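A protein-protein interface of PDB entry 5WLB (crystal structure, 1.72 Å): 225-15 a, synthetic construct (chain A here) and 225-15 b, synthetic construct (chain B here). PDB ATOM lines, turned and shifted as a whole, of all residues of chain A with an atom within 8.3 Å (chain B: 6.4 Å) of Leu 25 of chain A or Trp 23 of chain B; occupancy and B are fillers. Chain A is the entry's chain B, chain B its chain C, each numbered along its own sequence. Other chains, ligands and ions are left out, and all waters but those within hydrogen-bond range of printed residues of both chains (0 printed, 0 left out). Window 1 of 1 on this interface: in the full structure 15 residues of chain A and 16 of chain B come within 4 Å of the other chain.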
ATOM      1  N   ARG A   4      -7.286 -27.522 -23.196  1.00  0.00           N
ATOM      2  CA  ARG A   4      -6.128 -26.990 -23.916  1.00  0.00           C
ATOM      3  C   ARG A   4      -4.899 -27.020 -23.018  1.00  0.00           C
ATOM      4  O   ARG A   4      -4.872 -26.403 -21.951  1.00  0.00           O
ATOM      5  CB  ARG A   4      -6.366 -25.555 -24.394  1.00  0.00           C
ATOM      6  CG  ARG A   4      -7.558 -25.382 -25.307  1.00  0.00           C
ATOM      7  CD  ARG A   4      -7.917 -23.915 -25.401  1.00  0.00           C
ATOM      8  NE  ARG A   4      -8.490 -23.564 -26.694  1.00  0.00           N
ATOM      9  CZ  ARG A   4      -9.256 -22.498 -26.896  1.00  0.00           C
ATOM     10  NH1 ARG A   4      -9.739 -22.237 -28.108  1.00  0.00           N
ATOM     11  NH2 ARG A   4      -9.547 -21.697 -25.876  1.00  0.00           N
ATOM     12  N   ARG A   5      -3.888 -27.757 -23.438  1.00  0.00           N
ATOM     13  CA  ARG A   5      -2.646 -27.749 -22.693  1.00  0.00           C
ATOM     14  C   ARG A   5      -1.973 -26.413 -22.922  1.00  0.00           C
ATOM     15  O   ARG A   5      -1.751 -26.017 -24.059  1.00  0.00           O
ATOM     16  CB  ARG A   5      -1.727 -28.889 -23.130  1.00  0.00           C
ATOM     17  CG  ARG A   5      -0.410 -28.876 -22.372  1.00  0.00           C
ATOM     18  CD  ARG A   5       0.520 -29.953 -22.906  1.00  0.00           C
ATOM     19  NE  ARG A   5       0.039 -31.291 -22.597  1.00  0.00           N
ATOM     20  CZ  ARG A   5       0.812 -32.378 -22.589  1.00  0.00           C
ATOM     21  NH1 ARG A   5       0.291 -33.558 -22.288  1.00  0.00           N
ATOM     22  NH2 ARG A   5       2.108 -32.285 -22.860  1.00  0.00           N
ATOM     23  N   PRO A   6      -1.650 -25.702 -21.838  1.00  0.00           N
ATOM     24  CA  PRO A   6      -0.917 -24.447 -22.006  1.00  0.00           C
ATOM     25  C   PRO A   6       0.447 -24.679 -22.630  1.00  0.00           C
ATOM     26  O   PRO A   6       1.099 -25.656 -22.321  1.00  0.00           O
ATOM     27  CB  PRO A   6      -0.783 -23.915 -20.572  1.00  0.00           C
ATOM     28  CG  PRO A   6      -0.906 -25.137 -19.709  1.00  0.00           C
ATOM     29  CD  PRO A   6      -1.870 -26.045 -20.422  1.00  0.00           C
ATOM     30  N   ARG A   7       0.877 -23.789 -23.509  1.00  0.00           N
ATOM     31  CA  ARG A   7       2.183 -23.980 -24.113  1.00  0.00           C
ATOM     32  C   ARG A   7       3.265 -23.604 -23.116  1.00  0.00           C
ATOM     33  O   ARG A   7       3.072 -22.681 -22.318  1.00  0.00           O
ATOM     34  CB  ARG A   7       2.296 -23.156 -25.400  1.00  0.00           C
ATOM     35  CG  ARG A   7       1.795 -23.928 -26.620  1.00  0.00           C
ATOM     36  CD  ARG A   7       1.278 -23.024 -27.724  1.00  0.00           C
ATOM     37  NE  ARG A   7       2.319 -22.196 -28.332  1.00  0.00           N
ATOM     38  CZ  ARG A   7       3.121 -22.592 -29.317  1.00  0.00           C
ATOM     39  NH1 ARG A   7       4.019 -21.758 -29.816  1.00  0.00           N
ATOM     40  NH2 ARG A   7       3.029 -23.819 -29.805  1.00  0.00           N
ATOM     41  N   PRO A   9       6.149 -22.050 -21.219  1.00  0.00           N
ATOM     42  CA  PRO A   9       6.355 -20.595 -21.108  1.00  0.00           C
ATOM     43  C   PRO A   9       7.635 -20.070 -21.781  1.00  0.00           C
ATOM     44  O   PRO A   9       7.719 -18.879 -22.087  1.00  0.00           O
ATOM     45  CB  PRO A   9       6.420 -20.372 -19.594  1.00  0.00           C
ATOM     46  CG  PRO A   9       6.925 -21.688 -19.054  1.00  0.00           C
ATOM     47  CD  PRO A   9       6.331 -22.749 -19.934  1.00  0.00           C
ATOM     48  N   LEU A  18       5.437 -16.814 -16.058  1.00  0.00           N
ATOM     49  CA  LEU A  18       5.462 -18.108 -15.352  1.00  0.00           C
ATOM     50  C   LEU A  18       4.267 -18.258 -14.418  1.00  0.00           C
ATOM     51  O   LEU A  18       3.693 -19.339 -14.312  1.00  0.00           O
ATOM     52  CB  LEU A  18       6.755 -18.280 -14.551  1.00  0.00           C
ATOM     53  CG  LEU A  18       8.009 -18.381 -15.417  1.00  0.00           C
ATOM     54  CD1 LEU A  18       9.238 -18.522 -14.541  1.00  0.00           C
ATOM     55  CD2 LEU A  18       7.862 -19.578 -16.342  1.00  0.00           C
ATOM     56  N   HIS A  19       3.952 -17.197 -13.684  1.00  0.00           N
ATOM     57  CA  HIS A  19       2.775 -17.224 -12.832  1.00  0.00           C
ATOM     58  C   HIS A  19       1.498 -17.491 -13.647  1.00  0.00           C
ATOM     59  O   HIS A  19       0.649 -18.294 -13.251  1.00  0.00           O
ATOM     60  CB  HIS A  19       2.654 -15.918 -12.063  1.00  0.00           C
ATOM     61  CG  HIS A  19       3.360 -15.929 -10.744  1.00  0.00           C
ATOM     62  ND1 HIS A  19       2.914 -16.672  -9.676  1.00  0.00           N
ATOM     63  CD2 HIS A  19       4.491 -15.304 -10.330  1.00  0.00           C
ATOM     64  CE1 HIS A  19       3.726 -16.485  -8.643  1.00  0.00           C
ATOM     65  NE2 HIS A  19       4.684 -15.654  -9.014  1.00  0.00           N
ATOM     66  N   GLU A  20       1.349 -16.790 -14.764  1.00  0.00           N
ATOM     67  CA  GLU A  20       0.179 -16.995 -15.623  1.00  0.00           C
ATOM     68  C   GLU A  20       0.148 -18.440 -16.127  1.00  0.00           C
ATOM     69  O   GLU A  20      -0.906 -19.124 -16.107  1.00  0.00           O
ATOM     70  CB  GLU A  20       0.187 -16.004 -16.807  1.00  0.00           C
ATOM     71  CG  GLU A  20      -0.263 -14.630 -16.424  1.00  0.00           C
ATOM     72  CD  GLU A  20      -1.795 -14.461 -16.335  1.00  0.00           C
ATOM     73  OE1 GLU A  20      -2.571 -15.295 -16.881  1.00  0.00           O
ATOM     74  OE2 GLU A  20      -2.215 -13.451 -15.735  1.00  0.00           O
ATOM     75  N   TYR A  21       1.312 -18.926 -16.535  1.00  0.00           N
ATOM     76  CA  TYR A  21       1.384 -20.277 -17.040  1.00  0.00           C
ATOM     77  C   TYR A  21       1.031 -21.254 -15.916  1.00  0.00           C
ATOM     78  O   TYR A  21       0.286 -22.212 -16.146  1.00  0.00           O
ATOM     79  CB  TYR A  21       2.781 -20.591 -17.644  1.00  0.00           C
ATOM     80  CG  TYR A  21       2.978 -22.070 -17.878  1.00  0.00           C
ATOM     81  CD1 TYR A  21       2.549 -22.674 -19.063  1.00  0.00           C
ATOM     82  CD2 TYR A  21       3.544 -22.879 -16.897  1.00  0.00           C
ATOM     83  CE1 TYR A  21       2.712 -24.025 -19.271  1.00  0.00           C
ATOM     84  CE2 TYR A  21       3.687 -24.234 -17.086  1.00  0.00           C
ATOM     85  CZ  TYR A  21       3.272 -24.810 -18.274  1.00  0.00           C
ATOM     86  OH  TYR A  21       3.442 -26.163 -18.462  1.00  0.00           O
ATOM     87  N   TRP A  22       1.521 -20.992 -14.695  1.00  0.00           N
ATOM     88  CA  TRP A  22       1.335 -21.965 -13.606  1.00  0.00           C
ATOM     89  C   TRP A  22      -0.154 -22.128 -13.277  1.00  0.00           C
ATOM     90  O   TRP A  22      -0.645 -23.253 -13.080  1.00  0.00           O
ATOM     91  CB  TRP A  22       2.107 -21.549 -12.336  1.00  0.00           C
ATOM     92  CG  TRP A  22       1.958 -22.565 -11.231  1.00  0.00           C
ATOM     93  CD1 TRP A  22       2.763 -23.649 -11.002  1.00  0.00           C
ATOM     94  CD2 TRP A  22       0.912 -22.623 -10.256  1.00  0.00           C
ATOM     95  NE1 TRP A  22       2.288 -24.378  -9.928  1.00  0.00           N
ATOM     96  CE2 TRP A  22       1.168 -23.752  -9.434  1.00  0.00           C
ATOM     97  CE3 TRP A  22      -0.195 -21.809  -9.965  1.00  0.00           C
ATOM     98  CZ2 TRP A  22       0.346 -24.099  -8.374  1.00  0.00           C
ATOM     99  CZ3 TRP A  22      -1.014 -22.153  -8.928  1.00  0.00           C
ATOM    100  CH2 TRP A  22      -0.744 -23.304  -8.133  1.00  0.00           C
ATOM    101  N   ALA A  23      -0.881 -21.018 -13.234  1.00  0.00           N
ATOM    102  CA  ALA A  23      -2.315 -21.095 -12.940  1.00  0.00           C
ATOM    103  C   ALA A  23      -3.061 -21.885 -14.027  1.00  0.00           C
ATOM    104  O   ALA A  23      -4.019 -22.620 -13.735  1.00  0.00           O
ATOM    105  CB  ALA A  23      -2.909 -19.678 -12.774  1.00  0.00           C
ATOM    106  N   ARG A  24      -2.644 -21.712 -15.280  1.00  0.00           N
ATOM    107  CA  ARG A  24      -3.230 -22.484 -16.389  1.00  0.00           C
ATOM    108  C   ARG A  24      -2.888 -23.978 -16.263  1.00  0.00           C
ATOM    109  O   ARG A  24      -3.735 -24.844 -16.483  1.00  0.00           O
ATOM    110  CB  ARG A  24      -2.753 -21.946 -17.738  1.00  0.00           C
ATOM    111  CG  ARG A  24      -3.274 -20.526 -18.051  1.00  0.00           C
ATOM    112  CD  ARG A  24      -3.110 -20.196 -19.507  1.00  0.00           C
ATOM    113  NE  ARG A  24      -3.813 -21.202 -20.295  1.00  0.00           N
ATOM    114  CZ  ARG A  24      -3.629 -21.407 -21.592  1.00  0.00           C
ATOM    115  NH1 ARG A  24      -4.313 -22.365 -22.213  1.00  0.00           N
ATOM    116  NH2 ARG A  24      -2.757 -20.665 -22.260  1.00  0.00           N
ATOM    117  N   LEU A  25      -1.641 -24.277 -15.911  1.00  0.00           N
ATOM    118  CA  LEU A  25      -1.220 -25.667 -15.723  1.00  0.00           C
ATOM    119  C   LEU A  25      -1.966 -26.344 -14.561  1.00  0.00           C
ATOM    120  O   LEU A  25      -2.394 -27.495 -14.665  1.00  0.00           O
ATOM    121  CB  LEU A  25       0.301 -25.744 -15.517  1.00  0.00           C
ATOM    122  CG  LEU A  25       0.875 -27.170 -15.381  1.00  0.00           C
ATOM    123  CD1 LEU A  25       0.578 -27.987 -16.653  1.00  0.00           C
ATOM    124  CD2 LEU A  25       2.373 -27.129 -15.137  1.00  0.00           C
ATOM    125  N   TRP A  26      -2.155 -25.631 -13.457  1.00  0.00           N
ATOM    126  CA  TRP A  26      -2.962 -26.123 -12.351  1.00  0.00           C
ATOM    127  C   TRP A  26      -4.345 -26.594 -12.833  1.00  0.00           C
ATOM    128  O   TRP A  26      -4.810 -27.670 -12.475  1.00  0.00           O
ATOM    129  CB  TRP A  26      -3.084 -25.000 -11.304  1.00  0.00           C
ATOM    130  CG  TRP A  26      -3.619 -25.296  -9.926  1.00  0.00           C
ATOM    131  CD1 TRP A  26      -3.608 -26.500  -9.253  1.00  0.00           C
ATOM    132  CD2 TRP A  26      -4.222 -24.345  -9.025  1.00  0.00           C
ATOM    133  NE1 TRP A  26      -4.144 -26.331  -7.994  1.00  0.00           N
ATOM    134  CE2 TRP A  26      -4.541 -25.031  -7.840  1.00  0.00           C
ATOM    135  CE3 TRP A  26      -4.540 -22.981  -9.126  1.00  0.00           C
ATOM    136  CZ2 TRP A  26      -5.155 -24.395  -6.733  1.00  0.00           C
ATOM    137  CZ3 TRP A  26      -5.141 -22.342  -8.023  1.00  0.00           C
ATOM    138  CH2 TRP A  26      -5.456 -23.068  -6.857  1.00  0.00           C
ATOM    139  N   ASN A  27      -5.017 -25.774 -13.629  1.00  0.00           N
ATOM    140  CA  ASN A  27      -6.346 -26.112 -14.094  1.00  0.00           C
ATOM    141  C   ASN A  27      -6.323 -27.229 -15.136  1.00  0.00           C
ATOM    142  O   ASN A  27      -7.183 -28.115 -15.140  1.00  0.00           O
ATOM    143  CB  ASN A  27      -7.022 -24.862 -14.676  1.00  0.00           C
ATOM    144  CG  ASN A  27      -7.633 -23.995 -13.599  1.00  0.00           C
ATOM    145  OD1 ASN A  27      -8.799 -24.149 -13.245  1.00  0.00           O
ATOM    146  ND2 ASN A  27      -6.836 -23.107 -13.052  1.00  0.00           N
ATOM    147  N   TYR A  28      -5.346 -27.184 -16.025  1.00  0.00           N
ATOM    148  CA  TYR A  28      -5.207 -28.232 -17.044  1.00  0.00           C
ATOM    149  C   TYR A  28      -5.011 -29.617 -16.422  1.00  0.00           C
ATOM    150  O   TYR A  28      -5.667 -30.590 -16.804  1.00  0.00           O
ATOM    151  CB  TYR A  28      -4.031 -27.948 -17.943  1.00  0.00           C
ATOM    152  CG  TYR A  28      -3.735 -29.045 -18.940  1.00  0.00           C
ATOM    153  CD1 TYR A  28      -4.593 -29.282 -20.009  1.00  0.00           C
ATOM    154  CD2 TYR A  28      -2.613 -29.860 -18.800  1.00  0.00           C
ATOM    155  CE1 TYR A  28      -4.338 -30.290 -20.930  1.00  0.00           C
ATOM    156  CE2 TYR A  28      -2.346 -30.872 -19.717  1.00  0.00           C
ATOM    157  CZ  TYR A  28      -3.202 -31.073 -20.784  1.00  0.00           C
ATOM    158  OH  TYR A  28      -2.944 -32.060 -21.707  1.00  0.00           O
ATOM    159  N   LEU A  29      -4.043 -29.698 -15.515  1.00  0.00           N
ATOM    160  CA  LEU A  29      -3.763 -30.974 -14.839  1.00  0.00           C
ATOM    161  C   LEU A  29      -4.981 -31.457 -14.036  1.00  0.00           C
ATOM    162  O   LEU A  29      -5.280 -32.657 -13.996  1.00  0.00           O
ATOM    163  CB  LEU A  29      -2.546 -30.850 -13.924  1.00  0.00           C
ATOM    164  CG  LEU A  29      -1.208 -30.589 -14.602  1.00  0.00           C
ATOM    165  CD1 LEU A  29      -0.120 -30.328 -13.549  1.00  0.00           C
ATOM    166  CD2 LEU A  29      -0.802 -31.801 -15.499  1.00  0.00           C
ATOM    167  N   TYR A  30      -5.670 -30.542 -13.365  1.00  0.00           N
ATOM    168  CA  TYR A  30      -6.879 -30.910 -12.650  1.00  0.00           C
ATOM    169  C   TYR A  30      -7.889 -31.550 -13.620  1.00  0.00           C
ATOM    170  O   TYR A  30      -8.521 -32.570 -13.304  1.00  0.00           O
ATOM    171  CB  TYR A  30      -7.496 -29.688 -11.946  1.00  0.00           C
ATOM    172  CG  TYR A  30      -8.836 -30.020 -11.346  1.00  0.00           C
ATOM    173  CD1 TYR A  30      -9.982 -30.023 -12.139  1.00  0.00           C
ATOM    174  CD2 TYR A  30      -8.952 -30.408 -10.018  1.00  0.00           C
ATOM    175  CE1 TYR A  30     -11.186 -30.386 -11.634  1.00  0.00           C
ATOM    176  CE2 TYR A  30     -10.200 -30.761  -9.492  1.00  0.00           C
ATOM    177  CZ  TYR A  30     -11.291 -30.743 -10.317  1.00  0.00           C
ATOM    178  OH  TYR A  30     -12.528 -31.065  -9.856  1.00  0.00           O
ATOM    179  N   ARG A  31      -8.052 -30.927 -14.787  1.00  0.00           N
ATOM    180  CA  ARG A  31      -9.040 -31.394 -15.762  1.00  0.00           C
ATOM    181  C   ARG A  31      -8.703 -32.771 -16.331  1.00  0.00           C
ATOM    182  O   ARG A  31      -9.593 -33.592 -16.514  1.00  0.00           O
ATOM    183  CB  ARG A  31      -9.159 -30.402 -16.918  1.00  0.00           C
ATOM    184  CG  ARG A  31      -9.878 -29.129 -16.566  1.00  0.00           C
ATOM    185  CD  ARG A  31     -11.370 -29.339 -16.554  1.00  0.00           C
ATOM    186  NE  ARG A  31     -12.056 -28.253 -15.863  1.00  0.00           N
ATOM    187  CZ  ARG A  31     -13.284 -28.347 -15.363  1.00  0.00           C
ATOM    188  NH1 ARG A  31     -13.963 -29.482 -15.480  1.00  0.00           N
ATOM    189  NH2 ARG A  31     -13.827 -27.309 -14.744  1.00  0.00           N
ATOM    190  N   VAL A  32      -7.424 -33.018 -16.612  1.00  0.00           N
ATOM    191  CA  VAL A  32      -7.034 -34.248 -17.302  1.00  0.00           C
ATOM    192  C   VAL A  32      -6.766 -35.423 -16.353  1.00  0.00           C
ATOM    193  O   VAL A  32      -6.672 -36.561 -16.804  1.00  0.00           O
ATOM    194  CB  VAL A  32      -5.777 -34.046 -18.194  1.00  0.00           C
ATOM    195  CG1 VAL A  32      -5.934 -32.816 -19.067  1.00  0.00           C
ATOM    196  CG2 VAL A  32      -4.538 -33.936 -17.367  1.00  0.00           C
ATOM    197  N   GLN B  18       5.276 -35.990 -16.140  1.00  0.00           N
ATOM    198  CA  GLN B  18       6.311 -34.960 -16.215  1.00  0.00           C
ATOM    199  C   GLN B  18       5.762 -33.558 -15.913  1.00  0.00           C
ATOM    200  O   GLN B  18       6.408 -32.751 -15.251  1.00  0.00           O
ATOM    201  CB  GLN B  18       6.974 -34.974 -17.587  1.00  0.00           C
ATOM    202  CG  GLN B  18       7.947 -36.132 -17.768  1.00  0.00           C
ATOM    203  CD  GLN B  18       8.522 -36.193 -19.174  1.00  0.00           C
ATOM    204  OE1 GLN B  18       7.800 -36.049 -20.165  1.00  0.00           O
ATOM    205  NE2 GLN B  18       9.827 -36.398 -19.266  1.00  0.00           N
ATOM    206  N   LEU B  19       4.573 -33.253 -16.428  1.00  0.00           N
ATOM    207  CA  LEU B  19       3.981 -31.948 -16.147  1.00  0.00           C
ATOM    208  C   LEU B  19       3.556 -31.802 -14.691  1.00  0.00           C
ATOM    209  O   LEU B  19       3.544 -30.702 -14.149  1.00  0.00           O
ATOM    210  CB  LEU B  19       2.769 -31.698 -17.067  1.00  0.00           C
ATOM    211  CG  LEU B  19       3.064 -31.326 -18.518  1.00  0.00           C
ATOM    212  CD1 LEU B  19       1.763 -31.184 -19.326  1.00  0.00           C
ATOM    213  CD2 LEU B  19       3.868 -30.043 -18.573  1.00  0.00           C
ATOM    214  N   HIS B  20       3.149 -32.905 -14.071  1.00  0.00           N
ATOM    215  CA  HIS B  20       2.747 -32.868 -12.674  1.00  0.00           C
ATOM    216  C   HIS B  20       3.972 -32.531 -11.819  1.00  0.00           C
ATOM    217  O   HIS B  20       3.898 -31.750 -10.855  1.00  0.00           O
ATOM    218  CB  HIS B  20       2.132 -34.220 -12.288  1.00  0.00           C
ATOM    219  CG  HIS B  20       1.707 -34.321 -10.859  1.00  0.00           C
ATOM    220  ND1 HIS B  20       0.689 -33.564 -10.328  1.00  0.00           N
ATOM    221  CD2 HIS B  20       2.161 -35.106  -9.852  1.00  0.00           C
ATOM    222  CE1 HIS B  20       0.537 -33.868  -9.053  1.00  0.00           C
ATOM    223  NE2 HIS B  20       1.415 -34.805  -8.739  1.00  0.00           N
ATOM    224  N   ALA B  21       5.114 -33.096 -12.201  1.00  0.00           N
ATOM    225  CA  ALA B  21       6.373 -32.762 -11.544  1.00  0.00           C
ATOM    226  C   ALA B  21       6.723 -31.288 -11.756  1.00  0.00           C
ATOM    227  O   ALA B  21       7.101 -30.579 -10.824  1.00  0.00           O
ATOM    228  CB  ALA B  21       7.506 -33.677 -12.069  1.00  0.00           C
ATOM    229  N   TYR B  22       6.587 -30.832 -12.990  1.00  0.00           N
ATOM    230  CA  TYR B  22       6.933 -29.463 -13.351  1.00  0.00           C
ATOM    231  C   TYR B  22       6.028 -28.518 -12.567  1.00  0.00           C
ATOM    232  O   TYR B  22       6.484 -27.526 -11.988  1.00  0.00           O
ATOM    233  CB  TYR B  22       6.772 -29.257 -14.852  1.00  0.00           C
ATOM    234  CG  TYR B  22       7.091 -27.850 -15.313  1.00  0.00           C
ATOM    235  CD1 TYR B  22       8.319 -27.254 -15.022  1.00  0.00           C
ATOM    236  CD2 TYR B  22       6.166 -27.116 -16.016  1.00  0.00           C
ATOM    237  CE1 TYR B  22       8.607 -25.955 -15.442  1.00  0.00           C
ATOM    238  CE2 TYR B  22       6.447 -25.842 -16.450  1.00  0.00           C
ATOM    239  CZ  TYR B  22       7.666 -25.258 -16.151  1.00  0.00           C
ATOM    240  OH  TYR B  22       7.918 -23.984 -16.593  1.00  0.00           O
ATOM    241  N   TRP B  23       4.748 -28.877 -12.501  1.00  0.00           N
ATOM    242  CA  TRP B  23       3.782 -28.056 -11.748  1.00  0.00           C
ATOM    243  C   TRP B  23       4.223 -27.868 -10.284  1.00  0.00           C
ATOM    244  O   TRP B  23       4.126 -26.757  -9.737  1.00  0.00           O
ATOM    245  CB  TRP B  23       2.381 -28.682 -11.833  1.00  0.00           C
ATOM    246  CG  TRP B  23       1.354 -28.066 -10.894  1.00  0.00           C
ATOM    247  CD1 TRP B  23       0.601 -26.920 -11.120  1.00  0.00           C
ATOM    248  CD2 TRP B  23       0.928 -28.579  -9.628  1.00  0.00           C
ATOM    249  NE1 TRP B  23      -0.228 -26.701 -10.052  1.00  0.00           N
ATOM    250  CE2 TRP B  23      -0.027 -27.679  -9.109  1.00  0.00           C
ATOM    251  CE3 TRP B  23       1.284 -29.714  -8.854  1.00  0.00           C
ATOM    252  CZ2 TRP B  23      -0.648 -27.873  -7.867  1.00  0.00           C
ATOM    253  CZ3 TRP B  23       0.687 -29.886  -7.620  1.00  0.00           C
ATOM    254  CH2 TRP B  23      -0.275 -28.978  -7.138  1.00  0.00           C
ATOM    255  N   GLN B  24       4.714 -28.933  -9.642  1.00  0.00           N
ATOM    256  CA  GLN B  24       5.180 -28.795  -8.263  1.00  0.00           C
ATOM    257  C   GLN B  24       6.445 -27.948  -8.163  1.00  0.00           C
ATOM    258  O   GLN B  24       6.624 -27.159  -7.235  1.00  0.00           O
ATOM    259  CB  GLN B  24       5.479 -30.176  -7.653  1.00  0.00           C
ATOM    260  CG  GLN B  24       4.278 -31.089  -7.604  1.00  0.00           C
ATOM    261  CD  GLN B  24       4.696 -32.555  -7.402  1.00  0.00           C
ATOM    262  OE1 GLN B  24       4.576 -33.399  -8.300  1.00  0.00           O
ATOM    263  NE2 GLN B  24       5.208 -32.845  -6.235  1.00  0.00           N
ATOM    264  N   ARG B  25       7.379 -28.213  -9.063  1.00  0.00           N
ATOM    265  CA  ARG B  25       8.659 -27.521  -9.057  1.00  0.00           C
ATOM    266  C   ARG B  25       8.505 -26.035  -9.349  1.00  0.00           C
ATOM    267  O   ARG B  25       9.161 -25.195  -8.728  1.00  0.00           O
ATOM    268  CB  ARG B  25       9.582 -28.194 -10.069  1.00  0.00           C
ATOM    269  CG  ARG B  25       9.908 -29.613  -9.596  1.00  0.00           C
ATOM    270  CD  ARG B  25      10.405 -30.557 -10.689  1.00  0.00           C
ATOM    271  NE  ARG B  25      11.273 -29.960 -11.692  1.00  0.00           N
ATOM    272  CZ  ARG B  25      12.562 -29.687 -11.520  1.00  0.00           C
ATOM    273  NH1 ARG B  25      13.140 -29.897 -10.355  1.00  0.00           N
ATOM    274  NH2 ARG B  25      13.268 -29.177 -12.518  1.00  0.00           N
ATOM    275  N   LEU B  26       7.610 -25.718 -10.273  1.00  0.00           N
ATOM    276  CA  LEU B  26       7.402 -24.325 -10.654  1.00  0.00           C
ATOM    277  C   LEU B  26       6.698 -23.581  -9.502  1.00  0.00           C
ATOM    278  O   LEU B  26       7.041 -22.438  -9.194  1.00  0.00           O
ATOM    279  CB  LEU B  26       6.601 -24.230 -11.945  1.00  0.00           C
ATOM    280  CG  LEU B  26       6.335 -22.836 -12.498  1.00  0.00           C
ATOM    281  CD1 LEU B  26       7.648 -22.090 -12.743  1.00  0.00           C
ATOM    282  CD2 LEU B  26       5.514 -22.924 -13.789  1.00  0.00           C
ATOM    283  N   TYR B  27       5.746 -24.253  -8.848  1.00  0.00           N
ATOM    284  CA  TYR B  27       5.144 -23.722  -7.611  1.00  0.00           C
ATOM    285  C   TYR B  27       6.205 -23.368  -6.583  1.00  0.00           C
ATOM    286  O   TYR B  27       6.155 -22.304  -5.956  1.00  0.00           O
ATOM    287  CB  TYR B  27       4.168 -24.733  -6.986  1.00  0.00           C
ATOM    288  CG  TYR B  27       3.596 -24.299  -5.657  1.00  0.00           C
ATOM    289  CD1 TYR B  27       2.531 -23.405  -5.594  1.00  0.00           C
ATOM    290  CD2 TYR B  27       4.121 -24.779  -4.462  1.00  0.00           C
ATOM    291  CE1 TYR B  27       2.001 -23.009  -4.366  1.00  0.00           C
ATOM    292  CE2 TYR B  27       3.610 -24.389  -3.247  1.00  0.00           C
ATOM    293  CZ  TYR B  27       2.544 -23.509  -3.200  1.00  0.00           C
ATOM    294  OH  TYR B  27       2.038 -23.135  -1.978  1.00  0.00           O
ATOM    295  N   ALA B  28       7.144 -24.290  -6.384  1.00  0.00           N
ATOM    296  CA  ALA B  28       8.178 -24.084  -5.381  1.00  0.00           C
ATOM    297  C   ALA B  28       9.097 -22.942  -5.766  1.00  0.00           C
ATOM    298  O   ALA B  28       9.459 -22.120  -4.929  1.00  0.00           O
ATOM    299  CB  ALA B  28       8.983 -25.349  -5.179  1.00  0.00           C
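Of chain A, only Trp 22, Leu 25, Trp 26 and Leu 29 come within 4 Å of Trp 23 of chain B.
Of the printed residues of chain B, Tyr 21 of chain A touches Leu 19 (3.9 Å), Tyr 22 (3.3 Å) and Leu 26 (3.7 Å).
Of the printed residues of chain A, Leu 19 of chain B touches Arg 5, Tyr 21, Leu 25 and Leu 29.
Of the printed residues of chain A, Tyr 22 of chain B touches Pro 9, Tyr 21 and Leu 25.
Printed residues of chain B within 4 Å of Trp 26 of chain A: Trp 23.
Of the printed residues of chain A, Leu 26 of chain B touches Tyr 21 (3.7 Å) and Trp 22 (3.95 Å).
Ala 28 of chain B touches none of the printed residues of chain A.
Arg 7 of chain A touches none of the printed residues of chain B.
The nearest residue of chain A that does not touch Trp 23 of chain B is Asn 27 of chain A (6.0 Å).
Hydrophobic or aromatic side chains of chain A within 4 Å of the printed part of chain B: Pro 9, Tyr 21, Trp 22, Leu 25, Trp 26 and Leu 29.
Of the 11 printed residues of chain B, 6 touch a printed residue of chain A.
Hydrophobic or aromatic side chains of chain B that line the printed part of chain A: Leu 19, Tyr 22, Trp 23, Leu 26 and Tyr 27.
Among the printed residues, no Asp or Glu carboxylate lies within 4 Å of a Lys or Arg side-chain nitrogen of the other chain.
The indole nitrogen of Trp 22 of chain A lies within hydrogen-bond range of the backbone carbonyl oxygen of Trp 23 of chain B, 3.0 Å away.
The guanidinium group (NE) of Arg 5 of chain A is in hydrogen-bond range of the side-chain hydroxyl (OH) of Tyr 28 of chain A, 3.2 Å away.
O of His 20 of chain B lies close to OE1 of Gln 24 of chain B, at 3.1 Å.
Arg 5 of chain A touches Leu 19 of chain B (CZ to CD1, 3.6 Å).
Tyr 22 of chain B touches Tyr 21 of chain A.
Leu 26 of chain B touches Tyr 21 of chain A (CD2 to CD2, 3.7 Å).
Trp 22 of chain A touches Leu 26 of chain B (CB to CD2, 3.95 Å).
Tyr 27 of chain B touches Trp 22 of chain A (CB to NE1, 3.5 Å).
Leu 25 of chain A touches Leu 19 of chain B (CD2 to O, 3.9 Å).
CD2 of Leu 25 of chain A touches CD2 of Tyr 22 of chain B, 3.9 Å away.
Trp 23 of chain B touches Leu 25 of chain A.
NE1 of Trp 23 of chain B touches CD1 of Trp 26 of chain A, at 3.5 Å.
Trp 23 of chain B touches Leu 29 of chain A (CB to CD1, 3.5 Å).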
